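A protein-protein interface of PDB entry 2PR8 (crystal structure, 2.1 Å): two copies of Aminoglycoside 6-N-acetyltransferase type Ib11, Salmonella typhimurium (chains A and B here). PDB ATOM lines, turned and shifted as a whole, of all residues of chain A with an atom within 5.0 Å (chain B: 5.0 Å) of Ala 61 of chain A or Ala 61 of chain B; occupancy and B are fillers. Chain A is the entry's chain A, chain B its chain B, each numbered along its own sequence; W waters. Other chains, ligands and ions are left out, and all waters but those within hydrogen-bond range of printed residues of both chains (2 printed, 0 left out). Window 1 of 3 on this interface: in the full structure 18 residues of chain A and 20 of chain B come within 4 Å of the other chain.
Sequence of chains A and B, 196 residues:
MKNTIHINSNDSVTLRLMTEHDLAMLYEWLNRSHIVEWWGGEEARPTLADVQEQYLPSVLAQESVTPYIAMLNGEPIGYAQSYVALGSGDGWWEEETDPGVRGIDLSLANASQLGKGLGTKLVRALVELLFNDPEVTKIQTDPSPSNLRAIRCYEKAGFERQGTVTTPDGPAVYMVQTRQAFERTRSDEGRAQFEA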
ATOM      1  N   PRO A  57      -0.016  27.271  32.200  1.00  0.00           N
ATOM      2  CA  PRO A  57       0.733  26.374  31.311  1.00  0.00           C
ATOM      3  C   PRO A  57      -0.047  25.806  30.107  1.00  0.00           C
ATOM      4  O   PRO A  57       0.479  25.771  28.986  1.00  0.00           O
ATOM      5  CB  PRO A  57       1.221  25.288  32.273  1.00  0.00           C
ATOM      6  CG  PRO A  57       1.509  26.057  33.523  1.00  0.00           C
ATOM      7  CD  PRO A  57       0.295  27.014  33.619  1.00  0.00           C
ATOM      8  N   SER A  58      -1.272  25.319  30.332  1.00  0.00           N
ATOM      9  CA  SER A  58      -2.144  24.859  29.231  1.00  0.00           C
ATOM     10  C   SER A  58      -2.413  25.918  28.141  1.00  0.00           C
ATOM     11  O   SER A  58      -2.518  25.577  26.957  1.00  0.00           O
ATOM     12  CB  SER A  58      -3.465  24.408  29.797  1.00  0.00           C
ATOM     13  OG  SER A  58      -3.246  23.246  30.582  1.00  0.00           O
ATOM     14  N   VAL A  59      -2.521  27.184  28.527  1.00  0.00           N
ATOM     15  CA  VAL A  59      -2.716  28.228  27.526  1.00  0.00           C
ATOM     16  C   VAL A  59      -1.444  28.453  26.707  1.00  0.00           C
ATOM     17  O   VAL A  59      -1.510  28.704  25.518  1.00  0.00           O
ATOM     18  CB  VAL A  59      -3.201  29.610  28.087  1.00  0.00           C
ATOM     19  CG1 VAL A  59      -4.547  29.511  28.814  1.00  0.00           C
ATOM     20  CG2 VAL A  59      -2.208  30.219  28.971  1.00  0.00           C
ATOM     21  N   LEU A  60      -0.297  28.400  27.371  1.00  0.00           N
ATOM     22  CA  LEU A  60       1.005  28.565  26.699  1.00  0.00           C
ATOM     23  C   LEU A  60       1.283  27.396  25.756  1.00  0.00           C
ATOM     24  O   LEU A  60       1.852  27.562  24.666  1.00  0.00           O
ATOM     25  CB  LEU A  60       2.111  28.703  27.763  1.00  0.00           C
ATOM     26  CG  LEU A  60       2.043  30.008  28.569  1.00  0.00           C
ATOM     27  CD1 LEU A  60       3.176  30.053  29.595  1.00  0.00           C
ATOM     28  CD2 LEU A  60       2.099  31.231  27.647  1.00  0.00           C
ATOM     29  N   ALA A  61       0.818  26.207  26.157  1.00  0.00           N
ATOM     30  CA  ALA A  61       0.944  25.024  25.330  1.00  0.00           C
ATOM     31  C   ALA A  61       0.277  25.187  23.950  1.00  0.00           C
ATOM     32  O   ALA A  61       0.791  24.698  22.962  1.00  0.00           O
ATOM     33  CB  ALA A  61       0.411  23.800  26.066  1.00  0.00           C
ATOM     34  N   GLN A  62      -0.845  25.880  23.896  1.00  0.00           N
ATOM     35  CA  GLN A  62      -1.565  26.146  22.650  1.00  0.00           C
ATOM     36  C   GLN A  62      -0.718  26.943  21.662  1.00  0.00           C
ATOM     37  O   GLN A  62      -0.887  26.823  20.452  1.00  0.00           O
ATOM     38  CB  GLN A  62      -2.860  26.908  22.932  1.00  0.00           C
ATOM     39  CG  GLN A  62      -3.981  26.020  23.454  1.00  0.00           C
ATOM     40  CD  GLN A  62      -5.370  26.679  23.532  1.00  0.00           C
ATOM     41  OE1 GLN A  62      -5.508  27.815  23.985  1.00  0.00           O
ATOM     42  NE2 GLN A  62      -6.415  25.925  23.116  1.00  0.00           N
ATOM     43  N   GLU A  63       0.198  27.737  22.211  1.00  0.00           N
ATOM     44  CA  GLU A  63       1.069  28.621  21.434  1.00  0.00           C
ATOM     45  C   GLU A  63       2.482  28.091  21.313  1.00  0.00           C
ATOM     46  O   GLU A  63       3.352  28.803  20.830  1.00  0.00           O
ATOM     47  CB  GLU A  63       1.112  30.012  22.122  1.00  0.00           C
ATOM     48  CG  GLU A  63      -0.186  30.814  21.980  1.00  0.00           C
ATOM     49  CD  GLU A  63      -0.489  31.266  20.534  1.00  0.00           C
ATOM     50  OE1 GLU A  63       0.401  31.175  19.649  1.00  0.00           O
ATOM     51  OE2 GLU A  63      -1.631  31.726  20.280  1.00  0.00           O
ATOM     52  N   SER A  64       2.710  26.862  21.790  1.00  0.00           N
ATOM     53  CA  SER A  64       4.003  26.195  21.767  1.00  0.00           C
ATOM     54  C   SER A  64       5.029  27.016  22.586  1.00  0.00           C
ATOM     55  O   SER A  64       6.175  27.227  22.172  1.00  0.00           O
ATOM     56  CB  SER A  64       4.455  25.965  20.307  1.00  0.00           C
ATOM     57  OG  SER A  64       3.409  25.335  19.551  1.00  0.00           O
ATOM     58  N   VAL A  65       4.568  27.517  23.727  1.00  0.00           N
ATOM     59  CA  VAL A  65       5.430  28.191  24.671  1.00  0.00           C
ATOM     60  C   VAL A  65       5.561  27.346  25.920  1.00  0.00           C
ATOM     61  O   VAL A  65       4.566  26.819  26.440  1.00  0.00           O
ATOM     62  CB  VAL A  65       4.932  29.628  24.982  1.00  0.00           C
ATOM     63  CG1 VAL A  65       5.877  30.310  26.006  1.00  0.00           C
ATOM     64  CG2 VAL A  65       4.846  30.501  23.680  1.00  0.00           C
ATOM     65  N   THR A  66       6.788  27.222  26.401  1.00  0.00           N
ATOM     66  CA  THR A  66       7.076  26.499  27.638  1.00  0.00           C
ATOM     67  C   THR A  66       7.603  27.494  28.677  1.00  0.00           C
ATOM     68  O   THR A  66       8.565  28.211  28.395  1.00  0.00           O
ATOM     69  CB  THR A  66       8.160  25.433  27.384  1.00  0.00           C
ATOM     70  OG1 THR A  66       7.745  24.571  26.314  1.00  0.00           O
ATOM     71  CG2 THR A  66       8.431  24.583  28.637  1.00  0.00           C
ATOM     72  N   PRO A  67       6.975  27.527  29.876  1.00  0.00           N
ATOM     73  CA  PRO A  67       7.354  28.449  30.956  1.00  0.00           C
ATOM     74  C   PRO A  67       8.329  27.813  31.929  1.00  0.00           C
ATOM     75  O   PRO A  67       8.217  26.620  32.223  1.00  0.00           O
ATOM     76  CB  PRO A  67       6.040  28.703  31.670  1.00  0.00           C
ATOM     77  CG  PRO A  67       5.251  27.404  31.478  1.00  0.00           C
ATOM     78  CD  PRO A  67       5.797  26.705  30.249  1.00  0.00           C
ATOM     79  N   PRO B  57       0.554  19.754  32.754  1.00  0.00           N
ATOM     80  CA  PRO B  57       0.500  20.631  31.587  1.00  0.00           C
ATOM     81  C   PRO B  57       1.829  21.278  31.140  1.00  0.00           C
ATOM     82  O   PRO B  57       2.056  21.406  29.940  1.00  0.00           O
ATOM     83  CB  PRO B  57      -0.538  21.668  32.000  1.00  0.00           C
ATOM     84  CG  PRO B  57      -1.475  20.838  32.881  1.00  0.00           C
ATOM     85  CD  PRO B  57      -0.517  20.060  33.714  1.00  0.00           C
ATOM     86  N   SER B  58       2.701  21.685  32.072  1.00  0.00           N
ATOM     87  CA  SER B  58       3.996  22.280  31.669  1.00  0.00           C
ATOM     88  C   SER B  58       4.862  21.274  30.911  1.00  0.00           C
ATOM     89  O   SER B  58       5.620  21.668  30.003  1.00  0.00           O
ATOM     90  CB  SER B  58       4.766  22.806  32.894  1.00  0.00           C
ATOM     91  OG  SER B  58       3.944  23.673  33.674  1.00  0.00           O
ATOM     92  N   VAL B  59       4.792  19.996  31.299  1.00  0.00           N
ATOM     93  CA  VAL B  59       5.531  18.951  30.572  1.00  0.00           C
ATOM     94  C   VAL B  59       4.948  18.792  29.161  1.00  0.00           C
ATOM     95  O   VAL B  59       5.672  18.729  28.190  1.00  0.00           O
ATOM     96  CB  VAL B  59       5.556  17.584  31.281  1.00  0.00           C
ATOM     97  CG1 VAL B  59       6.381  17.643  32.599  1.00  0.00           C
ATOM     98  CG2 VAL B  59       4.190  17.189  31.618  1.00  0.00           C
ATOM     99  N   LEU B  60       3.624  18.761  29.053  1.00  0.00           N
ATOM    100  CA  LEU B  60       2.986  18.701  27.737  1.00  0.00           C
ATOM    101  C   LEU B  60       3.354  19.912  26.888  1.00  0.00           C
ATOM    102  O   LEU B  60       3.542  19.799  25.680  1.00  0.00           O
ATOM    103  CB  LEU B  60       1.453  18.534  27.876  1.00  0.00           C
ATOM    104  CG  LEU B  60       1.047  17.201  28.525  1.00  0.00           C
ATOM    105  CD1 LEU B  60      -0.477  17.013  28.582  1.00  0.00           C
ATOM    106  CD2 LEU B  60       1.685  16.021  27.795  1.00  0.00           C
ATOM    107  N   ALA B  61       3.471  21.083  27.518  1.00  0.00           N
ATOM    108  CA  ALA B  61       3.887  22.289  26.782  1.00  0.00           C
ATOM    109  C   ALA B  61       5.224  22.126  26.062  1.00  0.00           C
ATOM    110  O   ALA B  61       5.375  22.572  24.916  1.00  0.00           O
ATOM    111  CB  ALA B  61       3.921  23.512  27.695  1.00  0.00           C
ATOM    112  N   GLN B  62       6.186  21.469  26.717  1.00  0.00           N
ATOM    113  CA  GLN B  62       7.480  21.199  26.103  1.00  0.00           C
ATOM    114  C   GLN B  62       7.379  20.366  24.849  1.00  0.00           C
ATOM    115  O   GLN B  62       8.305  20.352  24.068  1.00  0.00           O
ATOM    116  CB  GLN B  62       8.375  20.373  27.024  1.00  0.00           C
ATOM    117  CG  GLN B  62       8.549  20.828  28.428  1.00  0.00           C
ATOM    118  CD  GLN B  62       9.601  19.958  29.111  1.00  0.00           C
ATOM    119  OE1 GLN B  62       9.307  18.856  29.528  1.00  0.00           O
ATOM    120  NE2 GLN B  62      10.834  20.452  29.190  1.00  0.00           N
ATOM    121  N   GLU B  63       6.274  19.623  24.704  1.00  0.00           N
ATOM    122  CA  GLU B  63       6.055  18.766  23.546  1.00  0.00           C
ATOM    123  C   GLU B  63       4.986  19.343  22.619  1.00  0.00           C
ATOM    124  O   GLU B  63       4.525  18.666  21.698  1.00  0.00           O
ATOM    125  CB  GLU B  63       5.687  17.331  23.999  1.00  0.00           C
ATOM    126  CG  GLU B  63       6.909  16.464  24.467  1.00  0.00           C
ATOM    127  CD  GLU B  63       8.038  16.295  23.417  1.00  0.00           C
ATOM    128  OE1 GLU B  63       7.846  16.584  22.208  1.00  0.00           O
ATOM    129  OE2 GLU B  63       9.157  15.874  23.815  1.00  0.00           O
ATOM    130  N   SER B  64       4.612  20.607  22.861  1.00  0.00           N
ATOM    131  CA  SER B  64       3.612  21.324  22.043  1.00  0.00           C
ATOM    132  C   SER B  64       2.252  20.589  22.009  1.00  0.00           C
ATOM    133  O   SER B  64       1.585  20.564  20.985  1.00  0.00           O
ATOM    134  CB  SER B  64       4.138  21.529  20.619  1.00  0.00           C
ATOM    135  OG  SER B  64       5.442  22.088  20.648  1.00  0.00           O
ATOM    136  N   VAL B  65       1.879  20.008  23.153  1.00  0.00           N
ATOM    137  CA  VAL B  65       0.631  19.297  23.351  1.00  0.00           C
ATOM    138  C   VAL B  65      -0.221  20.105  24.366  1.00  0.00           C
ATOM    139  O   VAL B  65       0.257  20.502  25.453  1.00  0.00           O
ATOM    140  CB  VAL B  65       0.895  17.839  23.812  1.00  0.00           C
ATOM    141  CG1 VAL B  65      -0.419  17.093  24.260  1.00  0.00           C
ATOM    142  CG2 VAL B  65       1.752  17.027  22.761  1.00  0.00           C
ATOM    143  N   THR B  66      -1.473  20.364  23.975  1.00  0.00           N
ATOM    144  CA  THR B  66      -2.450  21.047  24.819  1.00  0.00           C
ATOM    145  C   THR B  66      -3.439  20.010  25.322  1.00  0.00           C
ATOM    146  O   THR B  66      -4.034  19.299  24.494  1.00  0.00           O
ATOM    147  CB  THR B  66      -3.251  22.091  24.023  1.00  0.00           C
ATOM    148  OG1 THR B  66      -2.355  22.974  23.303  1.00  0.00           O
ATOM    149  CG2 THR B  66      -4.113  22.877  24.951  1.00  0.00           C
ATOM    150  N   PRO B  67      -3.602  19.903  26.669  1.00  0.00           N
ATOM    151  CA  PRO B  67      -4.560  18.993  27.281  1.00  0.00           C
ATOM    152  C   PRO B  67      -5.908  19.676  27.568  1.00  0.00           C
ATOM    153  O   PRO B  67      -5.931  20.843  27.941  1.00  0.00           O
ATOM    154  CB  PRO B  67      -3.841  18.578  28.569  1.00  0.00           C
ATOM    155  CG  PRO B  67      -3.154  19.852  29.021  1.00  0.00           C
ATOM    156  CD  PRO B  67      -2.787  20.584  27.701  1.00  0.00           C
HETATM  157  O   HOH W   1      -0.426  22.436  21.438  1.00  0.00           O
HETATM  158  O   HOH W   2       5.106  23.676  18.077  1.00  0.00           O
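The side-chain hydroxyl (OG1) of Thr 66 of chain B is in hydrogen-bond range of the backbone NH (N) of Gln 62 of chain A, at 3.3 Å. The side-chain hydroxyl (OG1) of Thr 66 of chain A lies within hydrogen-bond range of the backbone carbonyl oxygen (O) of Ala 61 of chain B. The backbone NH (N) of Gln 62 of chain B sits close to the side-chain hydroxyl (OG1) of Thr 66 of chain A (3.5 Å).
Water W1 lies within hydrogen-bond range of the side-chain hydroxyl of Thr 66 of chain B (2.7 Å), the backbone carbonyl oxygen of Ser 64 of chain B (2.8 Å) and the backbone carbonyl oxygen of Ala 61 of chain A (3.0 Å). Water W2 lies within hydrogen-bond range of the side-chain hydroxyl (OG) of Ser 64 of chain A (2.8 Å) and the side-chain hydroxyl (OG) of Ser 64 of chain B (3.0 Å).
Hydrophobic or aromatic side chains of chain A that line the printed part of chain B: Pro 57 and Ala 61. Printed residues of chain B that touch a printed residue of chain A: Pro 57, Ser 58, Ala 61, Gln 62, Ser 64, Val 65, Thr 66 and Pro 67. Among the printed residues, 12 pairs touch across the chains. Among the printed residues, no Asp or Glu carboxylate lies within 4 Å of a Lys or Arg side-chain nitrogen of the other chain.
Ala 61 of chain B touches its own counterpart, Ala 61 of chain A. Ala 61 of chain A touches Val 65 of chain B, and with the chains exchanged Val 65 of chain A touches Ala 61 of chain B. Ala 61 of chain A touches Thr 66 of chain B, and with the chains exchanged Thr 66 of chain A touches Ala 61 of chain B. Ser 64 of chain B touches its own counterpart, Ser 64 of chain A. Positions printed for both chains: 57, 58, 59, 60, 61, 62, 63, 64, 65, 66 and 67. Of the 12 pairs that touch across the chains among the printed residues, 10 have their exchanged pair printed and touching as well.
OG of Ser 58 of chain B touches CG of Pro 57 of chain A (3.4 Å). OG of Ser 58 of chain A touches CB of Pro 57 of chain B, at 3.4 Å. Ser 58 of chain A touches Thr 66 of chain B (O to CG2, 3.7 Å). Pro 67 of chain B touches Ser 58 of chain A (CG to OG, 3.7 Å). Ala 61 of chain A touches Ala 61 of chain B. Ala 61 of chain A touches Val 65 of chain B. Ala 61 of chain A touches Thr 66 of chain B (C to OG1, 3.5 Å). Ser 64 of chain A touches Ser 64 of chain B. O of Val 65 of chain A touches CB of Ala 61 of chain B, at 3.6 Å.
Ala 61 of chain A touches just these residues of chain B: Ala 61, Val 65 and Thr 66. Printed residues of chain A within 4 Å of Ala 61 of chain B: Ala 61, Val 65 and Thr 66. Printed residues of chain A within 4 Å of Ser 64 of chain B: Ser 64 (3.98 Å). Of the printed residues of chain A, Val 65 of chain B touches Ala 61 (3.4 Å). Printed residues of chain B within 4 Å of Val 65 of chain A: Ala 61. Of the printed residues of chain A, Pro 57 of chain B touches Ser 58. Val 59 of chain A touches none of the printed residues of chain B. Val 59 of chain B touches none of the printed residues of chain A. The nearest residue of chain A that does not touch Ala 61 of chain B is Pro 57 of chain A (4.3 Å).
The backbone carbonyl oxygen (O) of Leu 60 of chain A is in hydrogen-bond range of the backbone NH (N) of Val 65 of chain A. O of Leu 60 of chain B is in hydrogen-bond range of N of Val 65 of chain B (3.0 Å).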
